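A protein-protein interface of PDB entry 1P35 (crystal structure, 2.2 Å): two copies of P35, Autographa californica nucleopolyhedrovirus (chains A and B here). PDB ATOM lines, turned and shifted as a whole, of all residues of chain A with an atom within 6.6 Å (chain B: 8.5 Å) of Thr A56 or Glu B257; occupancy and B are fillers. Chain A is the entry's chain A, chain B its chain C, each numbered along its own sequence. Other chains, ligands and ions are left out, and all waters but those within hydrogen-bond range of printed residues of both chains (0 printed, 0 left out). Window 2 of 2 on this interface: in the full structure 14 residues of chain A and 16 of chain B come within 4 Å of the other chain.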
ATOM      1  N   GLU A  26      11.954 -22.058 -23.103  1.00  0.00           N
ATOM      2  CA  GLU A  26      12.346 -20.859 -23.835  1.00  0.00           C
ATOM      3  C   GLU A  26      11.136 -20.156 -24.479  1.00  0.00           C
ATOM      4  O   GLU A  26      10.228 -20.793 -25.028  1.00  0.00           O
ATOM      5  CB  GLU A  26      13.388 -21.196 -24.920  1.00  0.00           C
ATOM      6  CG  GLU A  26      13.791 -19.991 -25.774  1.00  0.00           C
ATOM      7  CD  GLU A  26      14.547 -20.413 -27.043  1.00  0.00           C
ATOM      8  OE1 GLU A  26      13.966 -21.150 -27.846  1.00  0.00           O
ATOM      9  OE2 GLU A  26      15.716 -20.011 -27.243  1.00  0.00           O
ATOM     10  N   LEU A  27      11.118 -18.839 -24.343  1.00  0.00           N
ATOM     11  CA  LEU A  27      10.093 -18.023 -24.900  1.00  0.00           C
ATOM     12  C   LEU A  27      10.709 -17.170 -26.007  1.00  0.00           C
ATOM     13  O   LEU A  27      11.694 -16.482 -25.767  1.00  0.00           O
ATOM     14  CB  LEU A  27       9.482 -17.086 -23.847  1.00  0.00           C
ATOM     15  CG  LEU A  27       8.507 -16.112 -24.524  1.00  0.00           C
ATOM     16  CD1 LEU A  27       7.280 -16.917 -25.003  1.00  0.00           C
ATOM     17  CD2 LEU A  27       8.028 -15.020 -23.560  1.00  0.00           C
ATOM     18  N   VAL A  28      10.108 -17.243 -27.202  1.00  0.00           N
ATOM     19  CA  VAL A  28      10.485 -16.476 -28.364  1.00  0.00           C
ATOM     20  C   VAL A  28       9.229 -15.634 -28.562  1.00  0.00           C
ATOM     21  O   VAL A  28       8.068 -16.139 -28.562  1.00  0.00           O
ATOM     22  CB  VAL A  28      10.802 -17.357 -29.600  1.00  0.00           C
ATOM     23  CG1 VAL A  28      10.937 -16.453 -30.837  1.00  0.00           C
ATOM     24  CG2 VAL A  28      12.151 -18.021 -29.434  1.00  0.00           C
ATOM     25  N   SER A  54      18.631 -16.435 -18.995  1.00  0.00           N
ATOM     26  CA  SER A  54      19.507 -15.826 -19.981  1.00  0.00           C
ATOM     27  C   SER A  54      18.725 -15.560 -21.256  1.00  0.00           C
ATOM     28  O   SER A  54      17.655 -16.109 -21.430  1.00  0.00           O
ATOM     29  CB  SER A  54      20.737 -16.686 -20.254  1.00  0.00           C
ATOM     30  OG  SER A  54      20.390 -17.968 -20.683  1.00  0.00           O
ATOM     31  N   VAL A  55      19.231 -14.666 -22.101  1.00  0.00           N
ATOM     32  CA  VAL A  55      18.573 -14.345 -23.358  1.00  0.00           C
ATOM     33  C   VAL A  55      19.222 -15.220 -24.388  1.00  0.00           C
ATOM     34  O   VAL A  55      20.391 -15.562 -24.267  1.00  0.00           O
ATOM     35  CB  VAL A  55      18.832 -12.904 -23.799  1.00  0.00           C
ATOM     36  CG1 VAL A  55      18.072 -11.916 -22.903  1.00  0.00           C
ATOM     37  CG2 VAL A  55      20.330 -12.641 -23.695  1.00  0.00           C
ATOM     38  N   THR A  56      18.485 -15.558 -25.426  1.00  0.00           N
ATOM     39  CA  THR A  56      19.079 -16.395 -26.433  1.00  0.00           C
ATOM     40  C   THR A  56      19.051 -15.667 -27.773  1.00  0.00           C
ATOM     41  O   THR A  56      18.520 -14.561 -27.875  1.00  0.00           O
ATOM     42  CB  THR A  56      18.330 -17.732 -26.493  1.00  0.00           C
ATOM     43  OG1 THR A  56      16.927 -17.499 -26.754  1.00  0.00           O
ATOM     44  CG2 THR A  56      18.470 -18.446 -25.179  1.00  0.00           C
ATOM     45  N   ARG A  57      19.684 -16.254 -28.773  1.00  0.00           N
ATOM     46  CA  ARG A  57      19.716 -15.696 -30.130  1.00  0.00           C
ATOM     47  C   ARG A  57      19.204 -16.819 -31.015  1.00  0.00           C
ATOM     48  O   ARG A  57      19.673 -17.961 -30.927  1.00  0.00           O
ATOM     49  CB  ARG A  57      21.152 -15.300 -30.537  1.00  0.00           C
ATOM     50  CG  ARG A  57      21.347 -14.664 -31.968  1.00  0.00           C
ATOM     51  CD  ARG A  57      20.527 -13.394 -32.174  1.00  0.00           C
ATOM     52  NE  ARG A  57      20.917 -12.579 -33.339  1.00  0.00           N
ATOM     53  CZ  ARG A  57      20.836 -12.931 -34.626  1.00  0.00           C
ATOM     54  NH1 ARG A  57      20.383 -14.123 -34.998  1.00  0.00           N
ATOM     55  NH2 ARG A  57      21.191 -12.055 -35.561  1.00  0.00           N
ATOM     56  N   LYS A  58      18.200 -16.512 -31.829  1.00  0.00           N
ATOM     57  CA  LYS A  58      17.639 -17.511 -32.726  1.00  0.00           C
ATOM     58  C   LYS A  58      18.070 -17.169 -34.127  1.00  0.00           C
ATOM     59  O   LYS A  58      18.490 -16.036 -34.393  1.00  0.00           O
ATOM     60  CB  LYS A  58      16.101 -17.529 -32.634  1.00  0.00           C
ATOM     61  CG  LYS A  58      15.586 -17.522 -31.218  1.00  0.00           C
ATOM     62  CD  LYS A  58      16.174 -18.635 -30.326  1.00  0.00           C
ATOM     63  CE  LYS A  58      15.883 -20.018 -30.844  1.00  0.00           C
ATOM     64  NZ  LYS A  58      16.469 -21.019 -29.910  1.00  0.00           N
ATOM     65  N   HIS A  99      15.989  -5.761 -31.456  1.00  0.00           N
ATOM     66  CA  HIS A  99      15.876  -6.579 -30.269  1.00  0.00           C
ATOM     67  C   HIS A  99      15.473  -5.814 -29.030  1.00  0.00           C
ATOM     68  O   HIS A  99      16.030  -4.753 -28.729  1.00  0.00           O
ATOM     69  CB  HIS A  99      17.189  -7.311 -30.012  1.00  0.00           C
ATOM     70  CG  HIS A  99      17.579  -8.226 -31.127  1.00  0.00           C
ATOM     71  ND1 HIS A  99      18.062  -7.766 -32.336  1.00  0.00           N
ATOM     72  CD2 HIS A  99      17.524  -9.573 -31.234  1.00  0.00           C
ATOM     73  CE1 HIS A  99      18.292  -8.791 -33.135  1.00  0.00           C
ATOM     74  NE2 HIS A  99      17.975  -9.900 -32.490  1.00  0.00           N
ATOM     75  N   LEU A 166      12.685 -10.941 -29.440  1.00  0.00           N
ATOM     76  CA  LEU A 166      13.325 -11.241 -28.161  1.00  0.00           C
ATOM     77  C   LEU A 166      13.154 -12.711 -27.940  1.00  0.00           C
ATOM     78  O   LEU A 166      12.262 -13.317 -28.508  1.00  0.00           O
ATOM     79  CB  LEU A 166      12.700 -10.488 -26.990  1.00  0.00           C
ATOM     80  CG  LEU A 166      11.263 -10.860 -26.546  1.00  0.00           C
ATOM     81  CD1 LEU A 166      11.287 -11.928 -25.482  1.00  0.00           C
ATOM     82  CD2 LEU A 166      10.576  -9.654 -25.936  1.00  0.00           C
ATOM     83  N   SER A 167      14.052 -13.284 -27.149  1.00  0.00           N
ATOM     84  CA  SER A 167      13.980 -14.678 -26.781  1.00  0.00           C
ATOM     85  C   SER A 167      14.823 -14.876 -25.523  1.00  0.00           C
ATOM     86  O   SER A 167      15.832 -14.225 -25.343  1.00  0.00           O
ATOM     87  CB  SER A 167      14.455 -15.586 -27.924  1.00  0.00           C
ATOM     88  OG  SER A 167      15.726 -15.196 -28.422  1.00  0.00           O
ATOM     89  N   PHE A 168      14.405 -15.780 -24.653  1.00  0.00           N
ATOM     90  CA  PHE A 168      15.148 -15.991 -23.441  1.00  0.00           C
ATOM     91  C   PHE A 168      14.718 -17.324 -22.818  1.00  0.00           C
ATOM     92  O   PHE A 168      13.653 -17.868 -23.168  1.00  0.00           O
ATOM     93  CB  PHE A 168      14.911 -14.789 -22.483  1.00  0.00           C
ATOM     94  CG  PHE A 168      13.441 -14.625 -22.041  1.00  0.00           C
ATOM     95  CD1 PHE A 168      12.819 -15.590 -21.248  1.00  0.00           C
ATOM     96  CD2 PHE A 168      12.680 -13.546 -22.494  1.00  0.00           C
ATOM     97  CE1 PHE A 168      11.440 -15.492 -20.922  1.00  0.00           C
ATOM     98  CE2 PHE A 168      11.324 -13.426 -22.183  1.00  0.00           C
ATOM     99  CZ  PHE A 168      10.701 -14.416 -21.394  1.00  0.00           C
ATOM    100  N   GLU A 169      15.573 -17.878 -21.961  1.00  0.00           N
ATOM    101  CA  GLU A 169      15.231 -19.101 -21.250  1.00  0.00           C
ATOM    102  C   GLU A 169      14.838 -18.735 -19.831  1.00  0.00           C
ATOM    103  O   GLU A 169      15.369 -17.795 -19.240  1.00  0.00           O
ATOM    104  CB  GLU A 169      16.400 -20.080 -21.189  1.00  0.00           C
ATOM    105  CG  GLU A 169      16.560 -20.889 -22.442  1.00  0.00           C
ATOM    106  CD  GLU A 169      17.854 -21.651 -22.475  1.00  0.00           C
ATOM    107  OE1 GLU A 169      18.192 -22.245 -21.445  1.00  0.00           O
ATOM    108  OE2 GLU A 169      18.516 -21.682 -23.528  1.00  0.00           O
ATOM    109  N   TYR B  81      22.662 -17.355 -38.571  1.00  0.00           N
ATOM    110  CA  TYR B  81      22.656 -16.545 -37.377  1.00  0.00           C
ATOM    111  C   TYR B  81      23.421 -15.243 -37.533  1.00  0.00           C
ATOM    112  O   TYR B  81      23.738 -14.611 -36.534  1.00  0.00           O
ATOM    113  CB  TYR B  81      23.219 -17.307 -36.179  1.00  0.00           C
ATOM    114  CG  TYR B  81      22.365 -18.479 -35.729  1.00  0.00           C
ATOM    115  CD1 TYR B  81      22.414 -19.687 -36.410  1.00  0.00           C
ATOM    116  CD2 TYR B  81      21.571 -18.404 -34.579  1.00  0.00           C
ATOM    117  CE1 TYR B  81      21.720 -20.791 -35.962  1.00  0.00           C
ATOM    118  CE2 TYR B  81      20.869 -19.520 -34.122  1.00  0.00           C
ATOM    119  CZ  TYR B  81      20.962 -20.711 -34.828  1.00  0.00           C
ATOM    120  OH  TYR B  81      20.354 -21.872 -34.410  1.00  0.00           O
ATOM    121  N   THR B 248      27.960 -26.219 -36.238  1.00  0.00           N
ATOM    122  CA  THR B 248      27.595 -25.692 -34.934  1.00  0.00           C
ATOM    123  C   THR B 248      28.699 -24.791 -34.421  1.00  0.00           C
ATOM    124  O   THR B 248      29.861 -25.012 -34.685  1.00  0.00           O
ATOM    125  CB  THR B 248      27.430 -26.825 -33.883  1.00  0.00           C
ATOM    126  OG1 THR B 248      26.421 -27.741 -34.318  1.00  0.00           O
ATOM    127  CG2 THR B 248      27.059 -26.231 -32.509  1.00  0.00           C
ATOM    128  N   THR B 249      28.305 -23.752 -33.721  1.00  0.00           N
ATOM    129  CA  THR B 249      29.239 -22.888 -33.085  1.00  0.00           C
ATOM    130  C   THR B 249      28.648 -22.849 -31.683  1.00  0.00           C
ATOM    131  O   THR B 249      27.520 -23.294 -31.474  1.00  0.00           O
ATOM    132  CB  THR B 249      29.305 -21.445 -33.708  1.00  0.00           C
ATOM    133  OG1 THR B 249      28.028 -20.796 -33.641  1.00  0.00           O
ATOM    134  CG2 THR B 249      29.796 -21.528 -35.147  1.00  0.00           C
ATOM    135  N   GLU B 250      29.426 -22.353 -30.731  1.00  0.00           N
ATOM    136  CA  GLU B 250      29.011 -22.217 -29.342  1.00  0.00           C
ATOM    137  C   GLU B 250      30.037 -21.340 -28.661  1.00  0.00           C
ATOM    138  O   GLU B 250      31.176 -21.211 -29.123  1.00  0.00           O
ATOM    139  CB  GLU B 250      29.021 -23.568 -28.655  1.00  0.00           C
ATOM    140  CG  GLU B 250      30.403 -24.133 -28.540  1.00  0.00           C
ATOM    141  CD  GLU B 250      30.420 -25.500 -27.910  1.00  0.00           C
ATOM    142  OE1 GLU B 250      29.714 -26.398 -28.426  1.00  0.00           O
ATOM    143  OE2 GLU B 250      31.149 -25.676 -26.909  1.00  0.00           O
ATOM    144  N   SER B 251      29.655 -20.702 -27.578  1.00  0.00           N
ATOM    145  CA  SER B 251      30.643 -19.928 -26.851  1.00  0.00           C
ATOM    146  C   SER B 251      30.139 -20.017 -25.456  1.00  0.00           C
ATOM    147  O   SER B 251      29.214 -19.261 -25.092  1.00  0.00           O
ATOM    148  CB  SER B 251      30.688 -18.475 -27.299  1.00  0.00           C
ATOM    149  OG  SER B 251      31.751 -17.810 -26.631  1.00  0.00           O
ATOM    150  N   SER B 252      30.701 -20.968 -24.698  1.00  0.00           N
ATOM    151  CA  SER B 252      30.298 -21.205 -23.296  1.00  0.00           C
ATOM    152  C   SER B 252      30.631 -20.035 -22.359  1.00  0.00           C
ATOM    153  O   SER B 252      30.499 -20.160 -21.130  1.00  0.00           O
ATOM    154  CB  SER B 252      30.926 -22.504 -22.760  1.00  0.00           C
ATOM    155  N   TRP B 253      31.076 -18.918 -22.951  1.00  0.00           N
ATOM    156  CA  TRP B 253      31.386 -17.683 -22.221  1.00  0.00           C
ATOM    157  C   TRP B 253      30.114 -17.301 -21.450  1.00  0.00           C
ATOM    158  O   TRP B 253      29.986 -17.621 -20.261  1.00  0.00           O
ATOM    159  CB  TRP B 253      31.769 -16.553 -23.210  1.00  0.00           C
ATOM    160  N   GLY B 254      29.176 -16.640 -22.138  1.00  0.00           N
ATOM    161  CA  GLY B 254      27.915 -16.244 -21.515  1.00  0.00           C
ATOM    162  C   GLY B 254      27.196 -17.449 -20.917  1.00  0.00           C
ATOM    163  O   GLY B 254      27.239 -17.665 -19.702  1.00  0.00           O
ATOM    164  N   LYS B 255      26.512 -18.224 -21.756  1.00  0.00           N
ATOM    165  CA  LYS B 255      25.836 -19.443 -21.304  1.00  0.00           C
ATOM    166  C   LYS B 255      26.120 -20.478 -22.375  1.00  0.00           C
ATOM    167  O   LYS B 255      26.335 -20.103 -23.526  1.00  0.00           O
ATOM    168  CB  LYS B 255      24.311 -19.256 -21.152  1.00  0.00           C
ATOM    169  CG  LYS B 255      23.815 -18.661 -19.805  1.00  0.00           C
ATOM    170  CD  LYS B 255      23.978 -17.142 -19.695  1.00  0.00           C
ATOM    171  CE  LYS B 255      23.385 -16.656 -18.377  1.00  0.00           C
ATOM    172  NZ  LYS B 255      23.255 -15.164 -18.257  1.00  0.00           N
ATOM    173  N   SER B 256      26.138 -21.761 -22.001  1.00  0.00           N
ATOM    174  CA  SER B 256      26.400 -22.844 -22.959  1.00  0.00           C
ATOM    175  C   SER B 256      25.325 -22.885 -24.064  1.00  0.00           C
ATOM    176  O   SER B 256      24.476 -23.799 -24.120  1.00  0.00           O
ATOM    177  CB  SER B 256      26.468 -24.207 -22.243  1.00  0.00           C
ATOM    178  OG  SER B 256      26.779 -25.260 -23.149  1.00  0.00           O
ATOM    179  N   GLU B 257      25.382 -21.880 -24.941  1.00  0.00           N
ATOM    180  CA  GLU B 257      24.455 -21.740 -26.058  1.00  0.00           C
ATOM    181  C   GLU B 257      25.059 -22.289 -27.366  1.00  0.00           C
ATOM    182  O   GLU B 257      26.197 -21.978 -27.724  1.00  0.00           O
ATOM    183  CB  GLU B 257      24.087 -20.254 -26.230  1.00  0.00           C
ATOM    184  CG  GLU B 257      22.999 -19.980 -27.296  1.00  0.00           C
ATOM    185  CD  GLU B 257      22.654 -18.490 -27.461  1.00  0.00           C
ATOM    186  OE1 GLU B 257      23.596 -17.694 -27.684  1.00  0.00           O
ATOM    187  OE2 GLU B 257      21.450 -18.124 -27.390  1.00  0.00           O
ATOM    188  N   LYS B 258      24.297 -23.130 -28.059  1.00  0.00           N
ATOM    189  CA  LYS B 258      24.748 -23.668 -29.334  1.00  0.00           C
ATOM    190  C   LYS B 258      23.830 -23.271 -30.505  1.00  0.00           C
ATOM    191  O   LYS B 258      22.584 -23.338 -30.436  1.00  0.00           O
ATOM    192  CB  LYS B 258      24.912 -25.196 -29.260  1.00  0.00           C
ATOM    193  CG  LYS B 258      26.025 -25.612 -28.279  1.00  0.00           C
ATOM    194  CD  LYS B 258      26.277 -27.127 -28.213  1.00  0.00           C
ATOM    195  CE  LYS B 258      26.746 -27.688 -29.560  1.00  0.00           C
ATOM    196  NZ  LYS B 258      27.122 -29.150 -29.528  1.00  0.00           N
ATOM    197  N   TYR B 259      24.464 -22.834 -31.582  1.00  0.00           N
ATOM    198  CA  TYR B 259      23.734 -22.446 -32.768  1.00  0.00           C
ATOM    199  C   TYR B 259      23.989 -23.533 -33.793  1.00  0.00           C
ATOM    200  O   TYR B 259      25.138 -23.933 -34.005  1.00  0.00           O
ATOM    201  CB  TYR B 259      24.239 -21.098 -33.339  1.00  0.00           C
ATOM    202  CG  TYR B 259      24.088 -19.887 -32.439  1.00  0.00           C
ATOM    203  CD1 TYR B 259      23.378 -19.952 -31.240  1.00  0.00           C
ATOM    204  CD2 TYR B 259      24.721 -18.681 -32.763  1.00  0.00           C
ATOM    205  CE1 TYR B 259      23.314 -18.874 -30.389  1.00  0.00           C
ATOM    206  CE2 TYR B 259      24.662 -17.586 -31.912  1.00  0.00           C
ATOM    207  CZ  TYR B 259      23.963 -17.693 -30.720  1.00  0.00           C
ATOM    208  OH  TYR B 259      23.957 -16.635 -29.834  1.00  0.00           O
ATOM    209  N   ASN B 260      22.916 -24.022 -34.408  1.00  0.00           N
ATOM    210  CA  ASN B 260      23.021 -25.005 -35.469  1.00  0.00           C
ATOM    211  C   ASN B 260      22.714 -24.260 -36.784  1.00  0.00           C
ATOM    212  O   ASN B 260      21.563 -23.886 -37.030  1.00  0.00           O
ATOM    213  CB  ASN B 260      22.053 -26.140 -35.205  1.00  0.00           C
ATOM    214  CG  ASN B 260      22.319 -26.774 -33.870  1.00  0.00           C
ATOM    215  OD1 ASN B 260      23.322 -27.478 -33.707  1.00  0.00           O
ATOM    216  ND2 ASN B 260      21.471 -26.472 -32.883  1.00  0.00           N
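No position is printed for both chains.
Of the 6 pairs that touch across the chains among the printed residues, none has its exchanged pair printed and touching as well.
Hydrophobic or aromatic side chains of chain B within 4 Å of the printed part of chain A: Tyr B81 and Tyr B259.
Of the 13 printed residues of chain A, 4 touch a printed residue of chain B.
Among the printed residues, no Asp or Glu carboxylate lies within 4 Å of a Lys or Arg side-chain nitrogen of the other chain.
The side-chain carboxylate (OE2) of Glu B257 is in hydrogen-bond range of the backbone NH (N) of Arg A57 (2.9 Å).
CB of Ser A54 touches CE of Lys B255, at 3.2 Å.
Thr A56 touches Glu B257.
NH1 of Arg A57 touches O of Tyr B81, 3.7 Å away.
CB of Arg A57 touches OH of Tyr B259 (3.2 Å).
Lys A58 touches Tyr B81 (C to CE2, 3.7 Å).
OE2 of Glu A26 lies within hydrogen-bond range of OG1 of Thr A56, 2.8 Å away.
OE2 of Glu A26 lies within salt-bridge range of NZ of Lys A58 (2.9 Å).
The backbone NH (N) of Glu A169 lies within hydrogen-bond range of the backbone carbonyl oxygen (O) of Ser A54.
O of Thr A56 lies within hydrogen-bond range of OG of Ser A167 (2.9 Å).
OH of Tyr B81 lies within hydrogen-bond range of N of Asn B260 (3.3 Å).
OE1 of Glu B257 lies within hydrogen-bond range of OH of Tyr B259 (2.4 Å).
No residue of chain B comes within 4 Å of Val A55.
Of chain B, only Glu B257 comes within 4 Å of Thr A56.
Of the printed residues of chain B, Lys A58 touches Tyr B81.
Of the printed residues of chain A, Tyr B81 touches Arg A57 and Lys A58.
Of the printed residues of chain A, Glu B257 touches Thr A56 (3.1 Å) and Arg A57 (2.9 Å).
Lys B258 touches none of the printed residues of chain A.
Asn B260 touches none of the printed residues of chain A.
The nearest printed residue of chain A that does not touch Lys B255 is Val A55 (5.6 Å).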
